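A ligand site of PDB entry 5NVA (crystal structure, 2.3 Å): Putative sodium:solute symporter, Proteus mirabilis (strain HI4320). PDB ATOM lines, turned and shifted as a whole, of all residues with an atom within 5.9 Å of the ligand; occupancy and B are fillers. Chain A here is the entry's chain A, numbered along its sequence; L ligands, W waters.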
ATOM      1  N   PHE A  55     -16.817 -13.144  21.773  1.00  0.00           N
ATOM      2  CA  PHE A  55     -17.879 -14.070  21.398  1.00  0.00           C
ATOM      3  C   PHE A  55     -17.516 -14.837  20.131  1.00  0.00           C
ATOM      4  O   PHE A  55     -17.647 -16.069  20.084  1.00  0.00           O
ATOM      5  CB  PHE A  55     -19.190 -13.294  21.198  1.00  0.00           C
ATOM      6  CG  PHE A  55     -20.349 -14.155  20.834  1.00  0.00           C
ATOM      7  CD1 PHE A  55     -20.917 -15.014  21.760  1.00  0.00           C
ATOM      8  CD2 PHE A  55     -20.879 -14.113  19.556  1.00  0.00           C
ATOM      9  CE1 PHE A  55     -21.992 -15.811  21.418  1.00  0.00           C
ATOM     10  CE2 PHE A  55     -21.951 -14.910  19.204  1.00  0.00           C
ATOM     11  CZ  PHE A  55     -22.504 -15.758  20.147  1.00  0.00           C
ATOM     12  N   THR A  57     -14.559 -15.309  18.938  1.00  0.00           N
ATOM     13  CA  THR A  57     -13.389 -16.144  19.183  1.00  0.00           C
ATOM     14  C   THR A  57     -13.792 -17.506  19.746  1.00  0.00           C
ATOM     15  O   THR A  57     -13.326 -18.545  19.280  1.00  0.00           O
ATOM     16  CB  THR A  57     -12.431 -15.440  20.149  1.00  0.00           C
ATOM     17  OG1 THR A  57     -11.769 -14.365  19.476  1.00  0.00           O
ATOM     18  CG2 THR A  57     -11.399 -16.409  20.701  1.00  0.00           C
ATOM     19  N   THR A  58     -14.681 -17.513  20.738  1.00  0.00           N
ATOM     20  CA  THR A  58     -15.031 -18.763  21.398  1.00  0.00           C
ATOM     21  C   THR A  58     -15.979 -19.597  20.558  1.00  0.00           C
ATOM     22  O   THR A  58     -15.874 -20.831  20.541  1.00  0.00           O
ATOM     23  CB  THR A  58     -15.648 -18.464  22.772  1.00  0.00           C
ATOM     24  OG1 THR A  58     -16.803 -17.636  22.617  1.00  0.00           O
ATOM     25  CG2 THR A  58     -14.639 -17.773  23.671  1.00  0.00           C
ATOM     26  N   LEU A  59     -16.921 -18.971  19.845  1.00  0.00           N
ATOM     27  CA  LEU A  59     -17.904 -19.702  19.050  1.00  0.00           C
ATOM     28  C   LEU A  59     -17.320 -19.994  17.675  1.00  0.00           C
ATOM     29  O   LEU A  59     -17.194 -19.103  16.838  1.00  0.00           O
ATOM     30  CB  LEU A  59     -19.205 -18.905  18.938  1.00  0.00           C
ATOM     31  CG  LEU A  59     -20.461 -19.675  18.522  1.00  0.00           C
ATOM     32  CD1 LEU A  59     -21.712 -18.983  19.029  1.00  0.00           C
ATOM     33  CD2 LEU A  59     -20.552 -19.876  17.008  1.00  0.00           C
ATOM     34  N   SER A  60     -16.980 -21.263  17.442  1.00  0.00           N
ATOM     35  CA  SER A  60     -16.385 -21.707  16.183  1.00  0.00           C
ATOM     36  C   SER A  60     -17.382 -22.550  15.400  1.00  0.00           C
ATOM     37  O   SER A  60     -18.574 -22.601  15.721  1.00  0.00           O
ATOM     38  CB  SER A  60     -15.096 -22.476  16.461  1.00  0.00           C
ATOM     39  OG  SER A  60     -15.366 -23.749  17.022  1.00  0.00           O
ATOM     40  N   SER A  61     -16.878 -23.229  14.366  1.00  0.00           N
ATOM     41  CA  SER A  61     -17.681 -24.213  13.656  1.00  0.00           C
ATOM     42  C   SER A  61     -18.071 -25.380  14.560  1.00  0.00           C
ATOM     43  O   SER A  61     -18.983 -26.140  14.212  1.00  0.00           O
ATOM     44  CB  SER A  61     -16.924 -24.733  12.430  1.00  0.00           C
ATOM     45  OG  SER A  61     -15.626 -25.185  12.786  1.00  0.00           O
ATOM     46  N   ILE A  62     -17.389 -25.546  15.696  1.00  0.00           N
ATOM     47  CA  ILE A  62     -17.785 -26.552  16.677  1.00  0.00           C
ATOM     48  C   ILE A  62     -19.212 -26.295  17.160  1.00  0.00           C
ATOM     49  O   ILE A  62     -20.093 -27.146  17.022  1.00  0.00           O
ATOM     50  CB  ILE A  62     -16.790 -26.577  17.854  1.00  0.00           C
ATOM     51  CG1 ILE A  62     -15.408 -27.034  17.380  1.00  0.00           C
ATOM     52  CG2 ILE A  62     -17.307 -27.474  18.966  1.00  0.00           C
ATOM     53  CD1 ILE A  62     -14.356 -27.000  18.462  1.00  0.00           C
ATOM     54  N   THR A  63     -19.447 -25.102  17.713  1.00  0.00           N
ATOM     55  CA  THR A  63     -20.793 -24.755  18.164  1.00  0.00           C
ATOM     56  C   THR A  63     -21.773 -24.704  16.993  1.00  0.00           C
ATOM     57  O   THR A  63     -22.893 -25.214  17.090  1.00  0.00           O
ATOM     58  CB  THR A  63     -20.772 -23.422  18.896  1.00  0.00           C
ATOM     59  OG1 THR A  63     -20.119 -23.567  20.161  1.00  0.00           O
ATOM     60  CG2 THR A  63     -22.190 -22.899  19.126  1.00  0.00           C
ATOM     61  N   PHE A  64     -21.354 -24.092  15.878  1.00  0.00           N
ATOM     62  CA  PHE A  64     -22.265 -23.869  14.760  1.00  0.00           C
ATOM     63  C   PHE A  64     -22.857 -25.172  14.241  1.00  0.00           C
ATOM     64  O   PHE A  64     -24.030 -25.223  13.868  1.00  0.00           O
ATOM     65  CB  PHE A  64     -21.538 -23.127  13.642  1.00  0.00           C
ATOM     66  CG  PHE A  64     -22.437 -22.317  12.749  1.00  0.00           C
ATOM     67  CD1 PHE A  64     -23.262 -22.945  11.832  1.00  0.00           C
ATOM     68  CD2 PHE A  64     -22.460 -20.938  12.842  1.00  0.00           C
ATOM     69  CE1 PHE A  64     -24.094 -22.203  11.014  1.00  0.00           C
ATOM     70  CE2 PHE A  64     -23.287 -20.187  12.026  1.00  0.00           C
ATOM     71  CZ  PHE A  64     -24.105 -20.820  11.111  1.00  0.00           C
ATOM     72  N   ILE A  67     -23.829 -28.136  18.027  1.00  0.00           N
ATOM     73  CA  ILE A  67     -24.898 -27.767  18.958  1.00  0.00           C
ATOM     74  C   ILE A  67     -26.257 -28.084  18.320  1.00  0.00           C
ATOM     75  O   ILE A  67     -27.101 -28.700  18.988  1.00  0.00           O
ATOM     76  CB  ILE A  67     -24.804 -26.300  19.392  1.00  0.00           C
ATOM     77  CG1 ILE A  67     -23.626 -26.111  20.365  1.00  0.00           C
ATOM     78  CG2 ILE A  67     -26.100 -25.838  20.034  1.00  0.00           C
ATOM     79  CD1 ILE A  67     -23.761 -26.911  21.636  1.00  0.00           C
ATOM     80  N   PHE A  78     -27.329 -28.815  27.431  1.00  0.00           N
ATOM     81  CA  PHE A  78     -26.000 -28.220  27.315  1.00  0.00           C
ATOM     82  C   PHE A  78     -26.043 -26.697  27.300  1.00  0.00           C
ATOM     83  O   PHE A  78     -25.008 -26.067  27.549  1.00  0.00           O
ATOM     84  CB  PHE A  78     -25.299 -28.734  26.048  1.00  0.00           C
ATOM     85  CG  PHE A  78     -24.562 -30.028  26.252  1.00  0.00           C
ATOM     86  CD1 PHE A  78     -25.127 -31.064  26.971  1.00  0.00           C
ATOM     87  CD2 PHE A  78     -23.298 -30.203  25.714  1.00  0.00           C
ATOM     88  CE1 PHE A  78     -24.452 -32.257  27.146  1.00  0.00           C
ATOM     89  CE2 PHE A  78     -22.610 -31.393  25.894  1.00  0.00           C
ATOM     90  CZ  PHE A  78     -23.191 -32.418  26.608  1.00  0.00           C
ATOM     91  N   GLY A  81     -24.475 -24.501  30.082  1.00  0.00           N
ATOM     92  CA  GLY A  81     -23.095 -24.036  30.043  1.00  0.00           C
ATOM     93  C   GLY A  81     -22.952 -22.642  29.474  1.00  0.00           C
ATOM     94  O   GLY A  81     -21.974 -21.942  29.769  1.00  0.00           O
ATOM     95  N   GLN A  82     -23.898 -22.218  28.636  1.00  0.00           N
ATOM     96  CA  GLN A  82     -23.866 -20.862  28.101  1.00  0.00           C
ATOM     97  C   GLN A  82     -24.073 -19.841  29.210  1.00  0.00           C
ATOM     98  O   GLN A  82     -23.330 -18.856  29.315  1.00  0.00           O
ATOM     99  CB  GLN A  82     -24.922 -20.694  27.014  1.00  0.00           C
ATOM    100  CG  GLN A  82     -24.818 -21.697  25.881  1.00  0.00           C
ATOM    101  CD  GLN A  82     -23.591 -21.466  25.016  1.00  0.00           C
ATOM    102  OE1 GLN A  82     -23.037 -20.364  24.985  1.00  0.00           O
ATOM    103  NE2 GLN A  82     -23.157 -22.502  24.316  1.00  0.00           N
ATOM    104  N   ALA A  85     -21.299 -19.478  31.694  1.00  0.00           N
ATOM    105  CA  ALA A  85     -20.227 -18.620  31.189  1.00  0.00           C
ATOM    106  C   ALA A  85     -20.518 -17.161  31.499  1.00  0.00           C
ATOM    107  O   ALA A  85     -19.595 -16.387  31.808  1.00  0.00           O
ATOM    108  CB  ALA A  85     -20.043 -18.829  29.687  1.00  0.00           C
ATOM    109  N   ARG A 135      -6.659 -26.944  18.022  1.00  0.00           N
ATOM    110  CA  ARG A 135      -7.961 -26.308  17.894  1.00  0.00           C
ATOM    111  C   ARG A 135      -8.160 -25.722  16.497  1.00  0.00           C
ATOM    112  O   ARG A 135      -9.241 -25.834  15.911  1.00  0.00           O
ATOM    113  CB  ARG A 135      -8.138 -25.223  18.962  1.00  0.00           C
ATOM    114  CG  ARG A 135      -9.422 -24.417  18.814  1.00  0.00           C
ATOM    115  CD  ARG A 135      -9.624 -23.458  19.975  1.00  0.00           C
ATOM    116  NE  ARG A 135     -10.609 -22.422  19.676  1.00  0.00           N
ATOM    117  CZ  ARG A 135     -11.928 -22.562  19.833  1.00  0.00           C
ATOM    118  NH1 ARG A 135     -12.426 -23.711  20.275  1.00  0.00           N
ATOM    119  NH2 ARG A 135     -12.739 -21.566  19.529  1.00  0.00           N
ATOM    120  N   ILE A 139     -10.969 -27.137  14.070  1.00  0.00           N
ATOM    121  CA  ILE A 139     -11.973 -26.211  13.537  1.00  0.00           C
ATOM    122  C   ILE A 139     -12.006 -26.268  12.017  1.00  0.00           C
ATOM    123  O   ILE A 139     -13.085 -26.315  11.402  1.00  0.00           O
ATOM    124  CB  ILE A 139     -11.695 -24.785  14.045  1.00  0.00           C
ATOM    125  CG1 ILE A 139     -12.096 -24.642  15.511  1.00  0.00           C
ATOM    126  CG2 ILE A 139     -12.432 -23.761  13.196  1.00  0.00           C
ATOM    127  CD1 ILE A 139     -11.595 -23.362  16.146  1.00  0.00           C
ATOM    128  N   PHE A 243     -18.994 -27.519  32.733  1.00  0.00           N
ATOM    129  CA  PHE A 243     -19.006 -26.256  31.998  1.00  0.00           C
ATOM    130  C   PHE A 243     -18.578 -25.083  32.869  1.00  0.00           C
ATOM    131  O   PHE A 243     -18.040 -24.095  32.361  1.00  0.00           O
ATOM    132  CB  PHE A 243     -20.390 -25.995  31.414  1.00  0.00           C
ATOM    133  CG  PHE A 243     -20.608 -26.646  30.074  1.00  0.00           C
ATOM    134  CD1 PHE A 243     -19.595 -26.673  29.125  1.00  0.00           C
ATOM    135  CD2 PHE A 243     -21.834 -27.237  29.770  1.00  0.00           C
ATOM    136  CE1 PHE A 243     -19.805 -27.274  27.895  1.00  0.00           C
ATOM    137  CE2 PHE A 243     -22.039 -27.829  28.543  1.00  0.00           C
ATOM    138  CZ  PHE A 243     -21.029 -27.856  27.603  1.00  0.00           C
ATOM    139  N   ASN A 247     -15.587 -22.968  31.503  1.00  0.00           N
ATOM    140  CA  ASN A 247     -15.731 -21.545  31.258  1.00  0.00           C
ATOM    141  C   ASN A 247     -14.688 -20.736  32.025  1.00  0.00           C
ATOM    142  O   ASN A 247     -14.188 -19.727  31.525  1.00  0.00           O
ATOM    143  CB  ASN A 247     -17.142 -21.093  31.626  1.00  0.00           C
ATOM    144  CG  ASN A 247     -18.194 -21.602  30.655  1.00  0.00           C
ATOM    145  OD1 ASN A 247     -17.935 -21.714  29.458  1.00  0.00           O
ATOM    146  ND2 ASN A 247     -19.375 -21.918  31.172  1.00  0.00           N
ATOM    147  N   GLN A 250     -11.779 -20.852  29.990  1.00  0.00           N
ATOM    148  CA  GLN A 250     -11.897 -20.049  28.777  1.00  0.00           C
ATOM    149  C   GLN A 250     -11.676 -18.568  29.045  1.00  0.00           C
ATOM    150  O   GLN A 250     -11.121 -17.861  28.194  1.00  0.00           O
ATOM    151  CB  GLN A 250     -13.277 -20.276  28.157  1.00  0.00           C
ATOM    152  CG  GLN A 250     -13.533 -19.487  26.885  1.00  0.00           C
ATOM    153  CD  GLN A 250     -12.649 -19.931  25.727  1.00  0.00           C
ATOM    154  OE1 GLN A 250     -11.511 -19.483  25.603  1.00  0.00           O
ATOM    155  NE2 GLN A 250     -13.177 -20.806  24.885  1.00  0.00           N
ATOM    156  N   VAL A 281     -23.969 -14.144  24.333  1.00  0.00           N
ATOM    157  CA  VAL A 281     -24.061 -15.507  24.847  1.00  0.00           C
ATOM    158  C   VAL A 281     -25.461 -15.810  25.341  1.00  0.00           C
ATOM    159  O   VAL A 281     -25.929 -16.947  25.264  1.00  0.00           O
ATOM    160  CB  VAL A 281     -22.996 -15.731  25.946  1.00  0.00           C
ATOM    161  CG1 VAL A 281     -23.144 -17.102  26.578  1.00  0.00           C
ATOM    162  CG2 VAL A 281     -21.596 -15.563  25.373  1.00  0.00           C
ATOM    163  N   PRO A 285     -26.723 -18.367  21.254  1.00  0.00           N
ATOM    164  CA  PRO A 285     -26.711 -19.841  21.387  1.00  0.00           C
ATOM    165  C   PRO A 285     -28.096 -20.465  21.461  1.00  0.00           C
ATOM    166  O   PRO A 285     -28.259 -21.619  21.066  1.00  0.00           O
ATOM    167  CB  PRO A 285     -25.922 -20.069  22.675  1.00  0.00           C
ATOM    168  CG  PRO A 285     -25.013 -18.902  22.749  1.00  0.00           C
ATOM    169  CD  PRO A 285     -25.810 -17.745  22.233  1.00  0.00           C
ATOM    170  N   SER A 343     -12.462 -17.815  14.900  1.00  0.00           N
ATOM    171  CA  SER A 343     -11.759 -18.570  15.937  1.00  0.00           C
ATOM    172  C   SER A 343     -10.329 -18.895  15.538  1.00  0.00           C
ATOM    173  O   SER A 343      -9.442 -18.903  16.402  1.00  0.00           O
ATOM    174  CB  SER A 343     -12.531 -19.853  16.268  1.00  0.00           C
ATOM    175  OG  SER A 343     -13.777 -19.563  16.868  1.00  0.00           O
HETATM  176  C1  LIG L   1     -16.561 -23.622  20.074  1.00  0.00           C
HETATM  177  C2  LIG L   1     -16.834 -23.455  21.575  1.00  0.00           C
HETATM  178  C3  LIG L   1     -16.924 -24.811  22.249  1.00  0.00           C
HETATM  179  C4  LIG L   1     -17.387 -24.701  23.649  1.00  0.00           C
HETATM  180  C5  LIG L   1     -18.650 -23.907  23.752  1.00  0.00           C
HETATM  181  C6  LIG L   1     -18.484 -22.524  23.127  1.00  0.00           C
HETATM  182  C7  LIG L   1     -19.774 -21.759  23.220  1.00  0.00           C
HETATM  183  C8  LIG L   1     -19.597 -20.397  22.556  1.00  0.00           C
HETATM  184  C9  LIG L   1     -20.864 -19.565  22.711  1.00  0.00           C
HETATM  185  C10 LIG L   1     -20.309 -24.240  25.650  1.00  0.00           C
HETATM  186  C11 LIG L   1     -20.723 -24.029  27.102  1.00  0.00           C
HETATM  187  N1  LIG L   1     -19.040 -23.713  25.170  1.00  0.00           N
HETATM  188  O1  LIG L   1     -15.390 -23.819  19.663  1.00  0.00           O
HETATM  189  O2  LIG L   1     -17.518 -23.549  19.252  1.00  0.00           O
HETATM  190  O3  LIG L   1     -15.805 -22.754  22.131  1.00  0.00           O
HETATM  191  O4  LIG L   1     -17.617 -26.045  24.168  1.00  0.00           O
HETATM  192  O5  LIG L   1     -18.092 -22.651  21.723  1.00  0.00           O
HETATM  193  O6  LIG L   1     -20.795 -22.470  22.581  1.00  0.00           O
HETATM  194  O7  LIG L   1     -18.524 -19.719  23.158  1.00  0.00           O
HETATM  195  O8  LIG L   1     -20.997 -19.184  24.057  1.00  0.00           O
HETATM  196  O9  LIG L   1     -21.013 -24.825  24.904  1.00  0.00           O
HETATM  197  O   HOH W   1     -16.886 -22.995  27.460  1.00  0.00           O
HETATM  198  O   HOH W   2     -23.698 -25.211  25.335  1.00  0.00           O
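An oxygen (O7) of the ligand is in hydrogen-bond range of the side-chain hydroxyl (OG1) of Thr 58, 2.8 Å away.
O1 of the ligand lies within salt-bridge range of NH1 of Arg 135, 3.0 Å away.
The side-chain amide oxygen (OE1) of Gln 82 lies within hydrogen-bond range of an oxygen (O8) of the ligand.
The backbone NH (N) of Ser 60 sits at hydrogen-bond distance from an oxygen (O2) of the ligand, at 3.0 Å.
An oxygen (O1) of the ligand sits at hydrogen-bond distance from the side-chain hydroxyl (OG) of Ser 60, at 2.6 Å.
An oxygen (O2) of the ligand sits at hydrogen-bond distance from the backbone NH (N) of Thr 63, 2.9 Å away.
The side-chain hydroxyl (OG1) of Thr 63 is in hydrogen-bond range of an oxygen (O5) of the ligand (2.7 Å).
The backbone carbonyl oxygen of Thr 58 is in hydrogen-bond range of an oxygen (O3) of the ligand.
OG1 of Thr 58 lies within hydrogen-bond range of O of Phe 55, at 3.1 Å.
NH2 of Arg 135 is in hydrogen-bond range of O of Thr 57 (3.1 Å).
NH2 of Arg 135 lies within hydrogen-bond range of OG of Ser 343.
The guanidinium group (NH2) of Arg 135 lies within hydrogen-bond range of the backbone carbonyl oxygen (O) of Thr 58 (3.4 Å).
The backbone NH (N) of Ile 62 lies close to the side-chain hydroxyl (OG) of Ser 60 (3.0 Å).
The backbone carbonyl oxygen of Leu 59 is in hydrogen-bond range of the side-chain hydroxyl of Ser 343.
O of Phe 243 is in hydrogen-bond range of ND2 of Asn 247, 2.8 Å away.
The backbone carbonyl oxygen (O) of Gly 81 is in hydrogen-bond range of the side-chain amide nitrogen (ND2) of Asn 247, 3.0 Å away.
Merely in contact with the ligand: Leu 59 (3.8 Å), Ile 62 (3.4 Å), Gly 81 (3.5 Å), Phe 243 (3.5 Å) and Val 281 (3.9 Å).
Hydrophobic or aromatic side chains that line the ligand: Leu 59, Ile 62, Phe 243 and Val 281.
Within 4 Å of the ligand: Thr 58, Leu 59, Ser 60, Ile 62, Thr 63, Gly 81, Gln 82, Arg 135, Phe 243 and Val 281.
Along chain A the residues within 4 Å of the ligand span positions 58 to 281.
The nearest printed residue that does not touch the ligand is Phe 55 (4.1 Å).
Water W2 lies within hydrogen-bond range of the backbone carbonyl oxygen of Phe 78, an oxygen (O9) of the ligand and the side-chain amide nitrogen of Gln 82.
Water W1 bridges OD1 of Asn 247 and N1 of the ligand.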
